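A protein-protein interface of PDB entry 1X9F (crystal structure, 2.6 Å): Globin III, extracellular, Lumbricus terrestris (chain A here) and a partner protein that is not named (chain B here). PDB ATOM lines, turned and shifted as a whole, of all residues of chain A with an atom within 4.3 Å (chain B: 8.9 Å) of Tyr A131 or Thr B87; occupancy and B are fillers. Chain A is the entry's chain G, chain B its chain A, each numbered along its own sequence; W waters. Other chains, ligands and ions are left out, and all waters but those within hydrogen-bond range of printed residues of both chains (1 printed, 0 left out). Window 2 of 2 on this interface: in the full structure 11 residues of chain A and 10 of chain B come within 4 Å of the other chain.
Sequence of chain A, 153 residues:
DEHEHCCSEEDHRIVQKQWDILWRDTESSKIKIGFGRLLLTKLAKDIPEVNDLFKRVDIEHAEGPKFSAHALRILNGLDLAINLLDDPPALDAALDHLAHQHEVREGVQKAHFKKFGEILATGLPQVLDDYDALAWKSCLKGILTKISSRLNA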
ATOM      1  N   GLN A  18     -37.482   6.246 -32.206  1.00  0.00           N
ATOM      2  CA  GLN A  18     -36.543   5.686 -33.172  1.00  0.00           C
ATOM      3  C   GLN A  18     -37.092   4.446 -33.848  1.00  0.00           C
ATOM      4  O   GLN A  18     -36.876   4.231 -35.043  1.00  0.00           O
ATOM      5  CB  GLN A  18     -35.199   5.409 -32.507  1.00  0.00           C
ATOM      6  CG  GLN A  18     -34.534   6.698 -32.077  1.00  0.00           C
ATOM      7  CD  GLN A  18     -33.219   6.500 -31.357  1.00  0.00           C
ATOM      8  OE1 GLN A  18     -32.412   7.429 -31.294  1.00  0.00           O
ATOM      9  NE2 GLN A  18     -32.996   5.313 -30.806  1.00  0.00           N
ATOM     10  N   ALA A 121     -28.863  -5.655 -30.819  1.00  0.00           N
ATOM     11  CA  ALA A 121     -28.142  -4.390 -30.654  1.00  0.00           C
ATOM     12  C   ALA A 121     -27.271  -4.067 -31.869  1.00  0.00           C
ATOM     13  O   ALA A 121     -27.036  -2.901 -32.181  1.00  0.00           O
ATOM     14  CB  ALA A 121     -27.297  -4.418 -29.385  1.00  0.00           C
ATOM     15  N   LEU A 124     -30.083  -3.359 -35.204  1.00  0.00           N
ATOM     16  CA  LEU A 124     -30.970  -2.190 -35.207  1.00  0.00           C
ATOM     17  C   LEU A 124     -30.359  -0.947 -35.854  1.00  0.00           C
ATOM     18  O   LEU A 124     -31.012  -0.304 -36.685  1.00  0.00           O
ATOM     19  CB  LEU A 124     -31.486  -1.874 -33.803  1.00  0.00           C
ATOM     20  CG  LEU A 124     -32.611  -2.787 -33.320  1.00  0.00           C
ATOM     21  CD1 LEU A 124     -32.724  -2.707 -31.810  1.00  0.00           C
ATOM     22  CD2 LEU A 124     -33.946  -2.444 -33.996  1.00  0.00           C
ATOM     23  N   PRO A 125     -29.131  -0.584 -35.473  1.00  0.00           N
ATOM     24  CA  PRO A 125     -28.449   0.537 -36.108  1.00  0.00           C
ATOM     25  C   PRO A 125     -28.212   0.340 -37.600  1.00  0.00           C
ATOM     26  O   PRO A 125     -28.074   1.324 -38.328  1.00  0.00           O
ATOM     27  CB  PRO A 125     -27.111   0.617 -35.364  1.00  0.00           C
ATOM     28  CG  PRO A 125     -26.947  -0.674 -34.690  1.00  0.00           C
ATOM     29  CD  PRO A 125     -28.319  -1.163 -34.388  1.00  0.00           C
ATOM     30  N   ASP A 129     -31.233   4.849 -38.806  1.00  0.00           N
ATOM     31  CA  ASP A 129     -30.095   5.757 -38.901  1.00  0.00           C
ATOM     32  C   ASP A 129     -30.043   6.738 -37.735  1.00  0.00           C
ATOM     33  O   ASP A 129     -29.219   7.655 -37.711  1.00  0.00           O
ATOM     34  CB  ASP A 129     -30.104   6.498 -40.230  1.00  0.00           C
ATOM     35  CG  ASP A 129     -31.289   7.428 -40.377  1.00  0.00           C
ATOM     36  OD1 ASP A 129     -32.078   7.603 -39.418  1.00  0.00           O
ATOM     37  OD2 ASP A 129     -31.507   8.037 -41.445  1.00  0.00           O
ATOM     38  N   ASP A 130     -30.941   6.542 -36.780  1.00  0.00           N
ATOM     39  CA  ASP A 130     -30.969   7.318 -35.557  1.00  0.00           C
ATOM     40  C   ASP A 130     -31.119   6.328 -34.411  1.00  0.00           C
ATOM     41  O   ASP A 130     -32.182   5.733 -34.241  1.00  0.00           O
ATOM     42  CB  ASP A 130     -32.146   8.290 -35.594  1.00  0.00           C
ATOM     43  CG  ASP A 130     -32.063   9.346 -34.519  1.00  0.00           C
ATOM     44  OD1 ASP A 130     -33.128   9.853 -34.108  1.00  0.00           O
ATOM     45  OD2 ASP A 130     -30.986   9.738 -34.023  1.00  0.00           O
ATOM     46  N   TYR A 131     -30.056   6.137 -33.637  1.00  0.00           N
ATOM     47  CA  TYR A 131     -30.019   5.035 -32.684  1.00  0.00           C
ATOM     48  C   TYR A 131     -29.233   5.356 -31.426  1.00  0.00           C
ATOM     49  O   TYR A 131     -28.001   5.401 -31.452  1.00  0.00           O
ATOM     50  CB  TYR A 131     -29.412   3.801 -33.361  1.00  0.00           C
ATOM     51  CG  TYR A 131     -29.365   2.585 -32.474  1.00  0.00           C
ATOM     52  CD1 TYR A 131     -30.519   1.848 -32.210  1.00  0.00           C
ATOM     53  CD2 TYR A 131     -28.163   2.157 -31.909  1.00  0.00           C
ATOM     54  CE1 TYR A 131     -30.481   0.719 -31.399  1.00  0.00           C
ATOM     55  CE2 TYR A 131     -28.115   1.029 -31.096  1.00  0.00           C
ATOM     56  CZ  TYR A 131     -29.277   0.319 -30.842  1.00  0.00           C
ATOM     57  OH  TYR A 131     -29.233  -0.795 -30.037  1.00  0.00           O
ATOM     58  N   ASP A 132     -29.938   5.566 -30.319  1.00  0.00           N
ATOM     59  CA  ASP A 132     -29.262   5.775 -29.054  1.00  0.00           C
ATOM     60  C   ASP A 132     -28.942   4.411 -28.466  1.00  0.00           C
ATOM     61  O   ASP A 132     -29.830   3.728 -27.939  1.00  0.00           O
ATOM     62  CB  ASP A 132     -30.126   6.600 -28.107  1.00  0.00           C
ATOM     63  CG  ASP A 132     -29.382   7.020 -26.862  1.00  0.00           C
ATOM     64  OD1 ASP A 132     -29.040   8.217 -26.754  1.00  0.00           O
ATOM     65  OD2 ASP A 132     -29.084   6.226 -25.944  1.00  0.00           O
ATOM     66  N   ALA A 133     -27.678   4.006 -28.581  1.00  0.00           N
ATOM     67  CA  ALA A 133     -27.259   2.684 -28.127  1.00  0.00           C
ATOM     68  C   ALA A 133     -27.544   2.475 -26.648  1.00  0.00           C
ATOM     69  O   ALA A 133     -27.906   1.372 -26.239  1.00  0.00           O
ATOM     70  CB  ALA A 133     -25.780   2.441 -28.429  1.00  0.00           C
ATOM     71  N   LEU A 134     -27.387   3.534 -25.857  1.00  0.00           N
ATOM     72  CA  LEU A 134     -27.544   3.439 -24.409  1.00  0.00           C
ATOM     73  C   LEU A 134     -28.988   3.197 -23.989  1.00  0.00           C
ATOM     74  O   LEU A 134     -29.264   2.293 -23.195  1.00  0.00           O
ATOM     75  CB  LEU A 134     -26.967   4.675 -23.718  1.00  0.00           C
ATOM     76  CG  LEU A 134     -25.444   4.654 -23.615  1.00  0.00           C
ATOM     77  CD1 LEU A 134     -24.906   5.964 -23.079  1.00  0.00           C
ATOM     78  CD2 LEU A 134     -24.965   3.473 -22.771  1.00  0.00           C
ATOM     79  N   TRP A 136     -31.509   2.114 -25.933  1.00  0.00           N
ATOM     80  CA  TRP A 136     -31.937   0.827 -26.471  1.00  0.00           C
ATOM     81  C   TRP A 136     -31.445  -0.335 -25.631  1.00  0.00           C
ATOM     82  O   TRP A 136     -32.217  -1.238 -25.318  1.00  0.00           O
ATOM     83  CB  TRP A 136     -31.510   0.663 -27.926  1.00  0.00           C
ATOM     84  CG  TRP A 136     -32.492   1.268 -28.850  1.00  0.00           C
ATOM     85  CD1 TRP A 136     -32.503   2.551 -29.298  1.00  0.00           C
ATOM     86  CD2 TRP A 136     -33.635   0.629 -29.429  1.00  0.00           C
ATOM     87  NE1 TRP A 136     -33.577   2.752 -30.130  1.00  0.00           N
ATOM     88  CE2 TRP A 136     -34.289   1.585 -30.230  1.00  0.00           C
ATOM     89  CE3 TRP A 136     -34.172  -0.664 -29.359  1.00  0.00           C
ATOM     90  CZ2 TRP A 136     -35.449   1.294 -30.952  1.00  0.00           C
ATOM     91  CZ3 TRP A 136     -35.325  -0.954 -30.078  1.00  0.00           C
ATOM     92  CH2 TRP A 136     -35.949   0.021 -30.864  1.00  0.00           C
ATOM     93  N   CYS B   7     -26.885   4.720 -16.809  1.00  0.00           N
ATOM     94  CA  CYS B   7     -26.749   6.125 -17.157  1.00  0.00           C
ATOM     95  C   CYS B   7     -27.896   6.516 -18.094  1.00  0.00           C
ATOM     96  O   CYS B   7     -27.837   6.256 -19.298  1.00  0.00           O
ATOM     97  CB  CYS B   7     -25.383   6.353 -17.812  1.00  0.00           C
ATOM     98  SG  CYS B   7     -25.075   8.014 -18.449  1.00  0.00           S
ATOM     99  N   SER B   8     -28.942   7.125 -17.534  1.00  0.00           N
ATOM    100  CA  SER B   8     -30.153   7.427 -18.300  1.00  0.00           C
ATOM    101  C   SER B   8     -29.925   8.550 -19.298  1.00  0.00           C
ATOM    102  O   SER B   8     -28.876   9.198 -19.306  1.00  0.00           O
ATOM    103  CB  SER B   8     -31.319   7.786 -17.370  1.00  0.00           C
ATOM    104  OG  SER B   8     -31.317   9.167 -17.035  1.00  0.00           O
ATOM    105  N   TYR B   9     -30.923   8.773 -20.138  1.00  0.00           N
ATOM    106  CA  TYR B   9     -30.874   9.863 -21.084  1.00  0.00           C
ATOM    107  C   TYR B   9     -30.940  11.208 -20.352  1.00  0.00           C
ATOM    108  O   TYR B   9     -30.241  12.156 -20.719  1.00  0.00           O
ATOM    109  CB  TYR B   9     -32.003   9.733 -22.104  1.00  0.00           C
ATOM    110  CG  TYR B   9     -31.836  10.692 -23.238  1.00  0.00           C
ATOM    111  CD1 TYR B   9     -31.133  10.327 -24.385  1.00  0.00           C
ATOM    112  CD2 TYR B   9     -32.346  11.989 -23.151  1.00  0.00           C
ATOM    113  CE1 TYR B   9     -30.955  11.220 -25.424  1.00  0.00           C
ATOM    114  CE2 TYR B   9     -32.173  12.891 -24.176  1.00  0.00           C
ATOM    115  CZ  TYR B   9     -31.477  12.500 -25.310  1.00  0.00           C
ATOM    116  OH  TYR B   9     -31.305  13.398 -26.338  1.00  0.00           O
ATOM    117  N   ARG B  12     -27.588  11.970 -18.820  1.00  0.00           N
ATOM    118  CA  ARG B  12     -26.611  12.440 -19.796  1.00  0.00           C
ATOM    119  C   ARG B  12     -26.846  13.904 -20.102  1.00  0.00           C
ATOM    120  O   ARG B  12     -25.904  14.675 -20.288  1.00  0.00           O
ATOM    121  CB  ARG B  12     -26.660  11.595 -21.066  1.00  0.00           C
ATOM    122  CG  ARG B  12     -26.010  10.238 -20.876  1.00  0.00           C
ATOM    123  CD  ARG B  12     -25.974   9.389 -22.120  1.00  0.00           C
ATOM    124  NE  ARG B  12     -27.230   8.673 -22.325  1.00  0.00           N
ATOM    125  CZ  ARG B  12     -27.816   8.499 -23.506  1.00  0.00           C
ATOM    126  NH1 ARG B  12     -27.280   9.011 -24.612  1.00  0.00           N
ATOM    127  NH2 ARG B  12     -28.954   7.827 -23.585  1.00  0.00           N
ATOM    128  N   LEU B  80     -15.258  12.564 -23.714  1.00  0.00           N
ATOM    129  CA  LEU B  80     -16.273  11.586 -23.310  1.00  0.00           C
ATOM    130  C   LEU B  80     -17.632  12.235 -23.109  1.00  0.00           C
ATOM    131  O   LEU B  80     -18.645  11.741 -23.620  1.00  0.00           O
ATOM    132  CB  LEU B  80     -15.865  10.852 -22.030  1.00  0.00           C
ATOM    133  CG  LEU B  80     -14.630   9.955 -22.124  1.00  0.00           C
ATOM    134  CD1 LEU B  80     -14.325   9.310 -20.777  1.00  0.00           C
ATOM    135  CD2 LEU B  80     -14.812   8.899 -23.201  1.00  0.00           C
ATOM    136  N   ASN B  82     -18.778  15.032 -24.292  1.00  0.00           N
ATOM    137  CA  ASN B  82     -19.307  15.493 -25.582  1.00  0.00           C
ATOM    138  C   ASN B  82     -19.636  14.383 -26.584  1.00  0.00           C
ATOM    139  O   ASN B  82     -19.964  14.654 -27.742  1.00  0.00           O
ATOM    140  CB  ASN B  82     -18.354  16.498 -26.231  1.00  0.00           C
ATOM    141  CG  ASN B  82     -18.502  17.890 -25.662  1.00  0.00           C
ATOM    142  OD1 ASN B  82     -19.194  18.729 -26.228  1.00  0.00           O
ATOM    143  ND2 ASN B  82     -17.853  18.144 -24.537  1.00  0.00           N
ATOM    144  N   LEU B  83     -19.534  13.139 -26.138  1.00  0.00           N
ATOM    145  CA  LEU B  83     -19.881  11.997 -26.958  1.00  0.00           C
ATOM    146  C   LEU B  83     -21.106  11.316 -26.371  1.00  0.00           C
ATOM    147  O   LEU B  83     -21.652  10.392 -26.976  1.00  0.00           O
ATOM    148  CB  LEU B  83     -18.705  11.022 -27.028  1.00  0.00           C
ATOM    149  CG  LEU B  83     -17.954  10.830 -28.352  1.00  0.00           C
ATOM    150  CD1 LEU B  83     -18.025  12.048 -29.296  1.00  0.00           C
ATOM    151  CD2 LEU B  83     -16.516  10.411 -28.099  1.00  0.00           C
ATOM    152  N   LEU B  84     -21.544  11.790 -25.203  1.00  0.00           N
ATOM    153  CA  LEU B  84     -22.720  11.233 -24.507  1.00  0.00           C
ATOM    154  C   LEU B  84     -23.994  11.229 -25.345  1.00  0.00           C
ATOM    155  O   LEU B  84     -24.983  10.586 -24.990  1.00  0.00           O
ATOM    156  CB  LEU B  84     -22.975  11.953 -23.180  1.00  0.00           C
ATOM    157  CG  LEU B  84     -21.991  11.624 -22.057  1.00  0.00           C
ATOM    158  CD1 LEU B  84     -22.268  12.479 -20.829  1.00  0.00           C
ATOM    159  CD2 LEU B  84     -22.014  10.129 -21.702  1.00  0.00           C
ATOM    160  N   ASP B  85     -23.963  11.940 -26.461  1.00  0.00           N
ATOM    161  CA  ASP B  85     -25.119  11.999 -27.336  1.00  0.00           C
ATOM    162  C   ASP B  85     -24.858  11.324 -28.689  1.00  0.00           C
ATOM    163  O   ASP B  85     -25.724  11.364 -29.573  1.00  0.00           O
ATOM    164  CB  ASP B  85     -25.534  13.457 -27.531  1.00  0.00           C
ATOM    165  CG  ASP B  85     -27.026  13.664 -27.391  1.00  0.00           C
ATOM    166  OD1 ASP B  85     -27.446  14.829 -27.235  1.00  0.00           O
ATOM    167  OD2 ASP B  85     -27.857  12.733 -27.414  1.00  0.00           O
ATOM    168  N   ASP B  86     -23.671  10.728 -28.848  1.00  0.00           N
ATOM    169  CA  ASP B  86     -23.284  10.025 -30.076  1.00  0.00           C
ATOM    170  C   ASP B  86     -22.780   8.665 -29.631  1.00  0.00           C
ATOM    171  O   ASP B  86     -21.586   8.361 -29.720  1.00  0.00           O
ATOM    172  CB  ASP B  86     -22.187  10.795 -30.817  1.00  0.00           C
ATOM    173  CG  ASP B  86     -22.740  11.919 -31.677  1.00  0.00           C
ATOM    174  OD1 ASP B  86     -22.797  13.074 -31.193  1.00  0.00           O
ATOM    175  OD2 ASP B  86     -23.154  11.739 -32.842  1.00  0.00           O
ATOM    176  N   THR B  87     -23.718   7.850 -29.154  1.00  0.00           N
ATOM    177  CA  THR B  87     -23.416   6.639 -28.393  1.00  0.00           C
ATOM    178  C   THR B  87     -22.572   5.597 -29.111  1.00  0.00           C
ATOM    179  O   THR B  87     -21.801   4.887 -28.463  1.00  0.00           O
ATOM    180  CB  THR B  87     -24.706   5.982 -27.891  1.00  0.00           C
ATOM    181  OG1 THR B  87     -25.586   5.746 -28.996  1.00  0.00           O
ATOM    182  CG2 THR B  87     -25.483   6.934 -26.992  1.00  0.00           C
ATOM    183  N   LEU B  88     -22.722   5.489 -30.430  1.00  0.00           N
ATOM    184  CA  LEU B  88     -21.907   4.537 -31.187  1.00  0.00           C
ATOM    185  C   LEU B  88     -20.462   4.999 -31.309  1.00  0.00           C
ATOM    186  O   LEU B  88     -19.543   4.193 -31.153  1.00  0.00           O
ATOM    187  CB  LEU B  88     -22.519   4.206 -32.556  1.00  0.00           C
ATOM    188  CG  LEU B  88     -23.782   3.335 -32.569  1.00  0.00           C
ATOM    189  CD1 LEU B  88     -24.310   3.202 -33.992  1.00  0.00           C
ATOM    190  CD2 LEU B  88     -23.548   1.956 -31.943  1.00  0.00           C
ATOM    191  N   VAL B  89     -20.263   6.292 -31.568  1.00  0.00           N
ATOM    192  CA  VAL B  89     -18.923   6.891 -31.543  1.00  0.00           C
ATOM    193  C   VAL B  89     -18.349   6.732 -30.140  1.00  0.00           C
ATOM    194  O   VAL B  89     -17.204   6.306 -29.978  1.00  0.00           O
ATOM    195  CB  VAL B  89     -18.943   8.396 -31.918  1.00  0.00           C
ATOM    196  CG1 VAL B  89     -17.537   8.983 -31.875  1.00  0.00           C
ATOM    197  CG2 VAL B  89     -19.566   8.607 -33.293  1.00  0.00           C
ATOM    198  N   LEU B  90     -19.162   7.073 -29.136  1.00  0.00           N
ATOM    199  CA  LEU B  90     -18.788   6.905 -27.730  1.00  0.00           C
ATOM    200  C   LEU B  90     -18.278   5.488 -27.450  1.00  0.00           C
ATOM    201  O   LEU B  90     -17.183   5.309 -26.911  1.00  0.00           O
ATOM    202  CB  LEU B  90     -19.959   7.256 -26.799  1.00  0.00           C
ATOM    203  CG  LEU B  90     -19.762   6.956 -25.302  1.00  0.00           C
ATOM    204  CD1 LEU B  90     -18.613   7.760 -24.708  1.00  0.00           C
ATOM    205  CD2 LEU B  90     -21.053   7.194 -24.514  1.00  0.00           C
ATOM    206  N   GLN B  91     -19.070   4.495 -27.841  1.00  0.00           N
ATOM    207  CA  GLN B  91     -18.739   3.093 -27.635  1.00  0.00           C
ATOM    208  C   GLN B  91     -17.366   2.753 -28.229  1.00  0.00           C
ATOM    209  O   GLN B  91     -16.524   2.158 -27.554  1.00  0.00           O
ATOM    210  CB  GLN B  91     -19.856   2.245 -28.249  1.00  0.00           C
ATOM    211  CG  GLN B  91     -19.766   0.745 -28.077  1.00  0.00           C
ATOM    212  CD  GLN B  91     -20.949   0.051 -28.741  1.00  0.00           C
ATOM    213  OE1 GLN B  91     -22.106   0.284 -28.369  1.00  0.00           O
ATOM    214  NE2 GLN B  91     -20.670  -0.787 -29.737  1.00  0.00           N
ATOM    215  N   SER B  92     -17.144   3.153 -29.478  1.00  0.00           N
ATOM    216  CA  SER B  92     -15.873   2.935 -30.147  1.00  0.00           C
ATOM    217  C   SER B  92     -14.728   3.636 -29.421  1.00  0.00           C
ATOM    218  O   SER B  92     -13.749   2.983 -29.051  1.00  0.00           O
ATOM    219  CB  SER B  92     -15.959   3.424 -31.587  1.00  0.00           C
ATOM    220  OG  SER B  92     -14.722   3.253 -32.250  1.00  0.00           O
ATOM    221  N   HIS B  93     -14.853   4.949 -29.207  1.00  0.00           N
ATOM    222  CA  HIS B  93     -13.805   5.707 -28.520  1.00  0.00           C
ATOM    223  C   HIS B  93     -13.448   5.154 -27.141  1.00  0.00           C
ATOM    224  O   HIS B  93     -12.288   5.203 -26.720  1.00  0.00           O
ATOM    225  CB  HIS B  93     -14.160   7.186 -28.353  1.00  0.00           C
ATOM    226  CG  HIS B  93     -13.153   7.923 -27.530  1.00  0.00           C
ATOM    227  ND1 HIS B  93     -11.832   8.020 -27.911  1.00  0.00           N
ATOM    228  CD2 HIS B  93     -13.243   8.529 -26.322  1.00  0.00           C
ATOM    229  CE1 HIS B  93     -11.156   8.680 -26.989  1.00  0.00           C
ATOM    230  NE2 HIS B  93     -11.989   9.004 -26.015  1.00  0.00           N
ATOM    231  N   LEU B  94     -14.448   4.646 -26.433  1.00  0.00           N
ATOM    232  CA  LEU B  94     -14.246   4.108 -25.092  1.00  0.00           C
ATOM    233  C   LEU B  94     -13.217   2.961 -25.085  1.00  0.00           C
ATOM    234  O   LEU B  94     -12.408   2.845 -24.159  1.00  0.00           O
ATOM    235  CB  LEU B  94     -15.595   3.656 -24.526  1.00  0.00           C
ATOM    236  CG  LEU B  94     -16.102   4.133 -23.159  1.00  0.00           C
ATOM    237  CD1 LEU B  94     -15.533   5.488 -22.734  1.00  0.00           C
ATOM    238  CD2 LEU B  94     -17.631   4.171 -23.192  1.00  0.00           C
ATOM    239  N   ARG B 141     -20.478   4.106 -15.539  1.00  0.00           N
ATOM    240  CA  ARG B 141     -20.736   3.424 -16.807  1.00  0.00           C
ATOM    241  C   ARG B 141     -19.542   3.593 -17.735  1.00  0.00           C
ATOM    242  O   ARG B 141     -19.127   2.632 -18.390  1.00  0.00           O
ATOM    243  CB  ARG B 141     -22.016   3.955 -17.479  1.00  0.00           C
ATOM    244  CG  ARG B 141     -22.594   3.050 -18.591  1.00  0.00           C
ATOM    245  CD  ARG B 141     -21.968   3.222 -19.982  1.00  0.00           C
ATOM    246  NE  ARG B 141     -22.242   2.080 -20.856  1.00  0.00           N
ATOM    247  CZ  ARG B 141     -21.669   1.867 -22.040  1.00  0.00           C
ATOM    248  NH1 ARG B 141     -20.772   2.718 -22.522  1.00  0.00           N
ATOM    249  NH2 ARG B 141     -21.995   0.793 -22.747  1.00  0.00           N
ATOM    250  N   LEU B 142     -18.999   4.811 -17.788  1.00  0.00           N
ATOM    251  CA  LEU B 142     -17.832   5.111 -18.620  1.00  0.00           C
ATOM    252  C   LEU B 142     -16.626   4.321 -18.147  1.00  0.00           C
ATOM    253  O   LEU B 142     -15.984   3.620 -18.933  1.00  0.00           O
ATOM    254  CB  LEU B 142     -17.517   6.613 -18.620  1.00  0.00           C
ATOM    255  CG  LEU B 142     -18.516   7.555 -19.306  1.00  0.00           C
ATOM    256  CD1 LEU B 142     -18.175   9.013 -19.003  1.00  0.00           C
ATOM    257  CD2 LEU B 142     -18.583   7.325 -20.823  1.00  0.00           C
HETATM  258  O   HOH W   1     -28.287  10.030 -28.558  1.00  0.00           O
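Hydrophobic or aromatic side chains of chain A within 4 Å of the printed part of chain B: Ala A133 and Leu A134. Of the 20 printed residues of chain B, 4 touch a printed residue of chain A. Printed residues of chain B that touch a printed residue of chain A: Tyr B9, Arg B12, Thr B87 and Arg B141. Hydrophobic or aromatic side chains of chain B that line the printed part of chain A: Tyr B9. Among the printed residues, Asp or Glu carboxylates within 4 Å of a Lys or Arg side-chain nitrogen of the other chain: Asp A132 with Arg B12 (2.9 Å).
Among the printed residues, merely in contact across the chains: Leu A134 with Arg B141 (3.6 Å), Leu A134 with Arg B12 (3.6 Å), Asp A132 with Thr B87 (3.7 Å) and Asp A132 with Tyr B9 (3.8 Å).
NE of Arg B12 sits close to O of Ser B8 (3.5 Å). NH1 of Arg B12 sits at hydrogen-bond distance from O of Leu B84, at 2.8 Å. The side-chain amide nitrogen (NE2) of Gln A18 lies close to the backbone NH (N) of Asp A132 (3.1 Å). OD2 of Asp A132 lies close to N of Leu A134 (3.2 Å).
No residue of chain B comes within 4 Å of Asp A130. Tyr A131 touches just one residue of chain B: Thr B87. Asp A132 touches just these residues of chain B: Tyr B9, Arg B12 and Thr B87. Ala A133 touches just one residue of chain B: Thr B87. Printed residues of chain B within 4 Å of Leu A134: Arg B12 (3.6 Å) and Arg B141 (3.6 Å). Of the printed residues of chain A, Tyr B9 touches Asp A132 (3.8 Å). Of the printed residues of chain A, Arg B12 touches Asp A132 (2.9 Å) and Leu A134 (3.6 Å). Thr B87 touches just these residues of chain A: Tyr A131 (3.5 Å), Asp A132 (3.7 Å) and Ala A133 (2.8 Å). Of the printed residues of chain A, Arg B141 touches Leu A134 (3.6 Å). The nearest residue of chain B that does not touch Tyr A131 is Leu B88 (4.5 Å).
Water W1 bridges the side-chain carboxylate of Asp A132 (2.7 Å) and the side-chain carboxylate of Asp B85 (3.0 Å).
NH2 of Arg B12 lies within salt-bridge range of OD2 of Asp A132 (2.9 Å). The backbone carbonyl oxygen (O) of Tyr A131 sits at hydrogen-bond distance from the side-chain hydroxyl (OG1) of Thr B87 (3.5 Å). OG1 of Thr B87 sits at hydrogen-bond distance from N of Ala A133, 2.8 Å away.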
